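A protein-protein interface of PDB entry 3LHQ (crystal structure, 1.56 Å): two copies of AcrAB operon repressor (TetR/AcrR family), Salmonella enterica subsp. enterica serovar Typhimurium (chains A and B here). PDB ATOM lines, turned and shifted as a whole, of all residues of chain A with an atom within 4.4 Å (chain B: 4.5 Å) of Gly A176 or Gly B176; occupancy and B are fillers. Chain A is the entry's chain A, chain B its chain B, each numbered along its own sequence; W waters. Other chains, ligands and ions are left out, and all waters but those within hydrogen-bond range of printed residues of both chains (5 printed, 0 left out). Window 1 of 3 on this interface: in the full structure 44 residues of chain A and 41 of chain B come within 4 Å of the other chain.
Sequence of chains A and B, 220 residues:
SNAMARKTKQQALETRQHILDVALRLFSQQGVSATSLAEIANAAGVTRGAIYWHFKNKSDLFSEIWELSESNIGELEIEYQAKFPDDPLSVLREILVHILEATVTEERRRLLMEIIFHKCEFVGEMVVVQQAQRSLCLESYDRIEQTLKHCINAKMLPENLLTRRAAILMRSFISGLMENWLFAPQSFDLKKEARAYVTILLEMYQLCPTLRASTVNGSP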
ATOM      1  N   SER A 172     -20.785 -17.927  10.888  1.00  0.00           N
ATOM      2  CA  SER A 172     -19.965 -16.850  11.420  1.00  0.00           C
ATOM      3  C   SER A 172     -19.393 -17.216  12.784  1.00  0.00           C
ATOM      4  O   SER A 172     -18.243 -16.928  13.070  1.00  0.00           O
ATOM      5  CB  SER A 172     -20.730 -15.517  11.447  1.00  0.00           C
ATOM      6  OG  SER A 172     -21.928 -15.637  12.179  1.00  0.00           O
ATOM      7  N   PHE A 173     -20.199 -17.874  13.599  1.00  0.00           N
ATOM      8  CA  PHE A 173     -19.752 -18.267  14.919  1.00  0.00           C
ATOM      9  C   PHE A 173     -18.551 -19.251  14.813  1.00  0.00           C
ATOM     10  O   PHE A 173     -17.504 -19.110  15.432  1.00  0.00           O
ATOM     11  CB  PHE A 173     -20.988 -18.876  15.565  1.00  0.00           C
ATOM     12  CG  PHE A 173     -20.823 -19.327  16.987  1.00  0.00           C
ATOM     13  CD1 PHE A 173     -21.359 -18.565  18.033  1.00  0.00           C
ATOM     14  CD2 PHE A 173     -20.261 -20.532  17.296  1.00  0.00           C
ATOM     15  CE1 PHE A 173     -21.261 -19.024  19.335  1.00  0.00           C
ATOM     16  CE2 PHE A 173     -20.110 -20.964  18.583  1.00  0.00           C
ATOM     17  CZ  PHE A 173     -20.613 -20.219  19.594  1.00  0.00           C
ATOM     18  N   ILE A 174     -18.684 -20.223  13.927  1.00  0.00           N
ATOM     19  CA  ILE A 174     -17.691 -21.269  13.767  1.00  0.00           C
ATOM     20  C   ILE A 174     -16.457 -20.766  13.021  1.00  0.00           C
ATOM     21  O   ILE A 174     -15.295 -20.945  13.466  1.00  0.00           O
ATOM     22  CB  ILE A 174     -18.349 -22.490  13.082  1.00  0.00           C
ATOM     23  CG1 ILE A 174     -19.447 -23.042  13.997  1.00  0.00           C
ATOM     24  CG2 ILE A 174     -17.332 -23.499  12.642  1.00  0.00           C
ATOM     25  CD1 ILE A 174     -18.930 -23.773  15.274  1.00  0.00           C
ATOM     26  N   SER A 175     -16.649 -19.992  11.948  1.00  0.00           N
ATOM     27  CA  SER A 175     -15.514 -19.437  11.226  1.00  0.00           C
ATOM     28  C   SER A 175     -14.773 -18.419  12.053  1.00  0.00           C
ATOM     29  O   SER A 175     -13.546 -18.338  11.990  1.00  0.00           O
ATOM     30  CB  SER A 175     -15.972 -18.922   9.864  1.00  0.00           C
ATOM     31  OG  SER A 175     -16.640 -17.758   9.994  1.00  0.00           O
ATOM     32  N   GLY A 176     -15.487 -17.615  12.852  1.00  0.00           N
ATOM     33  CA  GLY A 176     -14.779 -16.676  13.726  1.00  0.00           C
ATOM     34  C   GLY A 176     -13.865 -17.290  14.785  1.00  0.00           C
ATOM     35  O   GLY A 176     -12.756 -16.827  15.090  1.00  0.00           O
ATOM     36  N   LEU A 177     -14.368 -18.346  15.421  1.00  0.00           N
ATOM     37  CA  LEU A 177     -13.604 -19.088  16.355  1.00  0.00           C
ATOM     38  C   LEU A 177     -12.336 -19.670  15.676  1.00  0.00           C
ATOM     39  O   LEU A 177     -11.243 -19.548  16.230  1.00  0.00           O
ATOM     40  CB  LEU A 177     -14.425 -20.215  16.948  1.00  0.00           C
ATOM     41  CG  LEU A 177     -15.346 -19.792  18.092  1.00  0.00           C
ATOM     42  CD1 LEU A 177     -16.358 -20.931  18.305  1.00  0.00           C
ATOM     43  CD2 LEU A 177     -14.593 -19.401  19.397  1.00  0.00           C
ATOM     44  N   MET A 178     -12.482 -20.285  14.489  1.00  0.00           N
ATOM     45  CA  MET A 178     -11.350 -20.830  13.766  1.00  0.00           C
ATOM     46  C   MET A 178     -10.337 -19.734  13.441  1.00  0.00           C
ATOM     47  O   MET A 178      -9.131 -19.849  13.707  1.00  0.00           O
ATOM     48  CB  MET A 178     -11.801 -21.512  12.495  1.00  0.00           C
ATOM     49  CG  MET A 178     -12.476 -22.833  12.739  1.00  0.00           C
ATOM     50  SD  MET A 178     -12.805 -23.658  11.149  1.00  0.00           S
ATOM     51  CE  MET A 178     -14.465 -23.332  11.193  1.00  0.00           C
ATOM     52  N   GLU A 179     -10.816 -18.659  12.840  1.00  0.00           N
ATOM     53  CA  GLU A 179      -9.941 -17.573  12.418  1.00  0.00           C
ATOM     54  C   GLU A 179      -9.220 -16.916  13.581  1.00  0.00           C
ATOM     55  O   GLU A 179      -8.030 -16.691  13.497  1.00  0.00           O
ATOM     56  CB  GLU A 179     -10.673 -16.570  11.505  1.00  0.00           C
ATOM     57  CG  GLU A 179      -9.790 -15.523  10.922  1.00  0.00           C
ATOM     58  CD  GLU A 179      -9.399 -14.354  11.854  1.00  0.00           C
ATOM     59  OE1 GLU A 179     -10.254 -13.843  12.617  1.00  0.00           O
ATOM     60  OE2 GLU A 179      -8.253 -13.891  11.789  1.00  0.00           O
ATOM     61  N   ASN A 180      -9.931 -16.632  14.668  1.00  0.00           N
ATOM     62  CA  ASN A 180      -9.344 -15.951  15.793  1.00  0.00           C
ATOM     63  C   ASN A 180      -8.280 -16.876  16.414  1.00  0.00           C
ATOM     64  O   ASN A 180      -7.180 -16.423  16.811  1.00  0.00           O
ATOM     65  CB  ASN A 180     -10.424 -15.597  16.830  1.00  0.00           C
ATOM     66  CG  ASN A 180     -11.353 -14.372  16.474  1.00  0.00           C
ATOM     67  OD1 ASN A 180     -12.102 -13.975  17.367  1.00  0.00           O
ATOM     68  ND2 ASN A 180     -11.317 -13.801  15.292  1.00  0.00           N
ATOM     69  N   SER B 172     -15.114 -13.556  18.473  1.00  0.00           N
ATOM     70  CA  SER B 172     -15.308 -14.504  17.370  1.00  0.00           C
ATOM     71  C   SER B 172     -16.629 -14.267  16.655  1.00  0.00           C
ATOM     72  O   SER B 172     -16.718 -14.357  15.427  1.00  0.00           O
ATOM     73  CB  SER B 172     -15.297 -15.919  17.884  1.00  0.00           C
ATOM     74  OG  SER B 172     -14.003 -16.302  18.241  1.00  0.00           O
ATOM     75  N   PHE B 173     -17.659 -13.976  17.435  1.00  0.00           N
ATOM     76  CA  PHE B 173     -19.023 -13.728  16.861  1.00  0.00           C
ATOM     77  C   PHE B 173     -18.989 -12.545  15.933  1.00  0.00           C
ATOM     78  O   PHE B 173     -19.417 -12.612  14.782  1.00  0.00           O
ATOM     79  CB  PHE B 173     -19.963 -13.530  18.029  1.00  0.00           C
ATOM     80  CG  PHE B 173     -21.438 -13.449  17.725  1.00  0.00           C
ATOM     81  CD1 PHE B 173     -22.294 -14.527  17.999  1.00  0.00           C
ATOM     82  CD2 PHE B 173     -22.009 -12.225  17.346  1.00  0.00           C
ATOM     83  CE1 PHE B 173     -23.674 -14.396  17.787  1.00  0.00           C
ATOM     84  CE2 PHE B 173     -23.314 -12.080  17.150  1.00  0.00           C
ATOM     85  CZ  PHE B 173     -24.173 -13.139  17.355  1.00  0.00           C
ATOM     86  N   ILE B 174     -18.403 -11.466  16.408  1.00  0.00           N
ATOM     87  CA  ILE B 174     -18.320 -10.229  15.664  1.00  0.00           C
ATOM     88  C   ILE B 174     -17.344 -10.305  14.477  1.00  0.00           C
ATOM     89  O   ILE B 174     -17.719  -9.936  13.343  1.00  0.00           O
ATOM     90  CB  ILE B 174     -17.970  -9.083  16.608  1.00  0.00           C
ATOM     91  CG1 ILE B 174     -19.064  -8.990  17.712  1.00  0.00           C
ATOM     92  CG2 ILE B 174     -17.729  -7.820  15.810  1.00  0.00           C
ATOM     93  CD1 ILE B 174     -20.414  -8.445  17.223  1.00  0.00           C
ATOM     94  N   SER B 175     -16.119 -10.855  14.684  1.00  0.00           N
ATOM     95  CA  SER B 175     -15.148 -11.000  13.595  1.00  0.00           C
ATOM     96  C   SER B 175     -15.670 -11.951  12.504  1.00  0.00           C
ATOM     97  O   SER B 175     -15.507 -11.673  11.306  1.00  0.00           O
ATOM     98  CB  SER B 175     -13.738 -11.389  14.144  1.00  0.00           C
ATOM     99  OG  SER B 175     -13.694 -12.680  14.600  1.00  0.00           O
ATOM    100  N   GLY B 176     -16.324 -13.038  12.918  1.00  0.00           N
ATOM    101  CA  GLY B 176     -16.900 -14.002  11.951  1.00  0.00           C
ATOM    102  C   GLY B 176     -18.000 -13.369  11.057  1.00  0.00           C
ATOM    103  O   GLY B 176     -18.047 -13.585   9.844  1.00  0.00           O
ATOM    104  N   LEU B 177     -18.890 -12.539  11.636  1.00  0.00           N
ATOM    105  CA  LEU B 177     -19.887 -11.851  10.836  1.00  0.00           C
ATOM    106  C   LEU B 177     -19.228 -10.912   9.818  1.00  0.00           C
ATOM    107  O   LEU B 177     -19.639 -10.870   8.644  1.00  0.00           O
ATOM    108  CB  LEU B 177     -20.844 -11.070  11.752  1.00  0.00           C
ATOM    109  CG  LEU B 177     -21.924 -11.932  12.445  1.00  0.00           C
ATOM    110  CD1 LEU B 177     -22.539 -11.195  13.634  1.00  0.00           C
ATOM    111  CD2 LEU B 177     -22.998 -12.460  11.439  1.00  0.00           C
ATOM    112  N   MET B 178     -18.270 -10.114  10.293  1.00  0.00           N
ATOM    113  CA  MET B 178     -17.560  -9.192   9.432  1.00  0.00           C
ATOM    114  C   MET B 178     -16.884  -9.940   8.318  1.00  0.00           C
ATOM    115  O   MET B 178     -17.016  -9.584   7.151  1.00  0.00           O
ATOM    116  CB  MET B 178     -16.560  -8.358  10.234  1.00  0.00           C
ATOM    117  CG  MET B 178     -17.233  -7.467  11.273  1.00  0.00           C
ATOM    118  SD  MET B 178     -16.039  -6.575  12.307  1.00  0.00           S
ATOM    119  CE  MET B 178     -14.968  -5.794  11.137  1.00  0.00           C
ATOM    120  N   GLU B 179     -16.127 -10.972   8.690  1.00  0.00           N
ATOM    121  CA  GLU B 179     -15.323 -11.702   7.683  1.00  0.00           C
ATOM    122  C   GLU B 179     -16.217 -12.366   6.631  1.00  0.00           C
ATOM    123  O   GLU B 179     -15.887 -12.360   5.436  1.00  0.00           O
ATOM    124  CB  GLU B 179     -14.353 -12.699   8.306  1.00  0.00           C
ATOM    125  CG  GLU B 179     -13.427 -13.336   7.296  1.00  0.00           C
ATOM    126  CD  GLU B 179     -14.010 -14.521   6.538  1.00  0.00           C
ATOM    127  OE1 GLU B 179     -14.791 -15.317   7.139  1.00  0.00           O
ATOM    128  OE2 GLU B 179     -13.630 -14.690   5.369  1.00  0.00           O
ATOM    129  N   ASN B 180     -17.278 -13.039   7.102  1.00  0.00           N
ATOM    130  CA  ASN B 180     -18.175 -13.805   6.267  1.00  0.00           C
ATOM    131  C   ASN B 180     -18.897 -12.834   5.326  1.00  0.00           C
ATOM    132  O   ASN B 180     -19.041 -13.107   4.135  1.00  0.00           O
ATOM    133  CB  ASN B 180     -19.218 -14.590   7.023  1.00  0.00           C
ATOM    134  CG  ASN B 180     -18.708 -15.864   7.730  1.00  0.00           C
ATOM    135  OD1 ASN B 180     -19.560 -16.623   8.233  1.00  0.00           O
ATOM    136  ND2 ASN B 180     -17.409 -16.152   7.705  1.00  0.00           N
HETATM  137  O   HOH W   1     -14.293 -15.786   9.899  1.00  0.00           O
HETATM  138  O   HOH W   2     -12.037 -14.792  20.044  1.00  0.00           O
HETATM  139  O   HOH W   3     -18.144 -17.344  17.633  1.00  0.00           O
HETATM  140  O   HOH W   4     -13.037 -13.943  11.766  1.00  0.00           O
HETATM  141  O   HOH W   5     -21.281 -14.853  14.725  1.00  0.00           O
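Of the printed residues of chain B, Ser A172 touches Ser B172 (3.8 Å), Gly B176 (3.4 Å), Leu B177 (3.4 Å) and Asn B180 (3.2 Å).
Phe A173 touches none of the printed residues of chain B.
Ile A174 touches none of the printed residues of chain B.
Printed residues of chain B within 4 Å of Gly A176: Ser B172 and Gly B176.
Printed residues of chain A within 4 Å of Ser B175: Asn A180 (2.7 Å).
Of the printed residues of chain A, Gly B176 touches Ser A172 (3.4 Å) and Gly A176 (3.8 Å).
Of the printed residues of chain A, Asn B180 touches Ser A172 (3.2 Å) and Ser A175 (2.9 Å).
The nearest printed residue of chain B that does not touch Gly A176 is Ser B175 (4.2 Å).
The nearest printed residue of chain A that does not touch Gly B176 is Ser A175 (4.2 Å).
The nearest printed residue of chain B that does not touch Asn A180 is Phe B173 (5.6 Å).
Ser B172 touches Ser A172 (O to O, 3.8 Å).
Gly B176 touches Ser A172.
CD2 of Leu B177 touches OG of Ser A172 (3.4 Å).
Gly B176 touches Gly A176 (CA to CA, 3.8 Å).
CD2 of Leu A177 touches OG of Ser B172 (3.4 Å).
The side-chain amide nitrogen (ND2) of Asn A180 sits close to the backbone carbonyl oxygen (O) of Gly A176, 3.4 Å away.
The side-chain carboxylate (OE1) of Glu A179 lies within hydrogen-bond range of the side-chain amide nitrogen (ND2) of Asn A180 (2.9 Å).
ND2 of Asn B180 lies close to O of Gly B176.
The side-chain carboxylate (OE1) of Glu B179 sits at hydrogen-bond distance from the side-chain amide nitrogen (ND2) of Asn B180, 2.8 Å away.
Hydrophobic or aromatic side chains of chain A that line the printed part of chain B: Leu A177.
Hydrophobic or aromatic side chains of chain B that line the printed part of chain A: Leu B177.
Among the printed residues, 10 pairs touch across the chains.
Ser B172 touches its own counterpart, Ser A172.
Ser A172 touches Asn B180, and with the chains exchanged Asn A180 touches Ser B172.
Ser A175 touches Asn B180, and with the chains exchanged Asn A180 touches Ser B175.
Gly A176 touches its own counterpart, Gly B176.
9 positions are printed for both chains.
Of the 10 pairs that touch across the chains among the printed residues, 10 have their exchanged pair printed and touching as well.
Water W5 lies within hydrogen-bond range of OG of Ser A172 (2.7 Å), O of Phe B173 (2.9 Å) and N of Phe A173 (3.4 Å).
Water W2 bridges OD1 of Asn A180 (2.8 Å) and OG of Ser B172 (3.1 Å).
Water W1 lies within hydrogen-bond range of the side-chain carboxylate of Glu B179 and the side-chain hydroxyl of Ser A175.
Water W3 lies within hydrogen-bond range of O of Phe A173 (2.9 Å) and N of Phe B173 (3.4 Å).
Water W4 lies within hydrogen-bond range of OE1 of Glu A179 (2.9 Å) and OG of Ser B175 (3.2 Å).
N of Ser A172 lies within hydrogen-bond range of OD1 of Asn B180 (3.2 Å).
The side-chain hydroxyl (OG) of Ser A175 lies within hydrogen-bond range of the side-chain amide nitrogen (ND2) of Asn B180.
OG of Ser B172 sits at hydrogen-bond distance from O of Gly A176.
The side-chain amide oxygen (OD1) of Asn A180 lies within hydrogen-bond range of the side-chain hydroxyl (OG) of Ser B172 (3.1 Å).
ND2 of Asn A180 is in hydrogen-bond range of OG of Ser B175 (2.7 Å).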
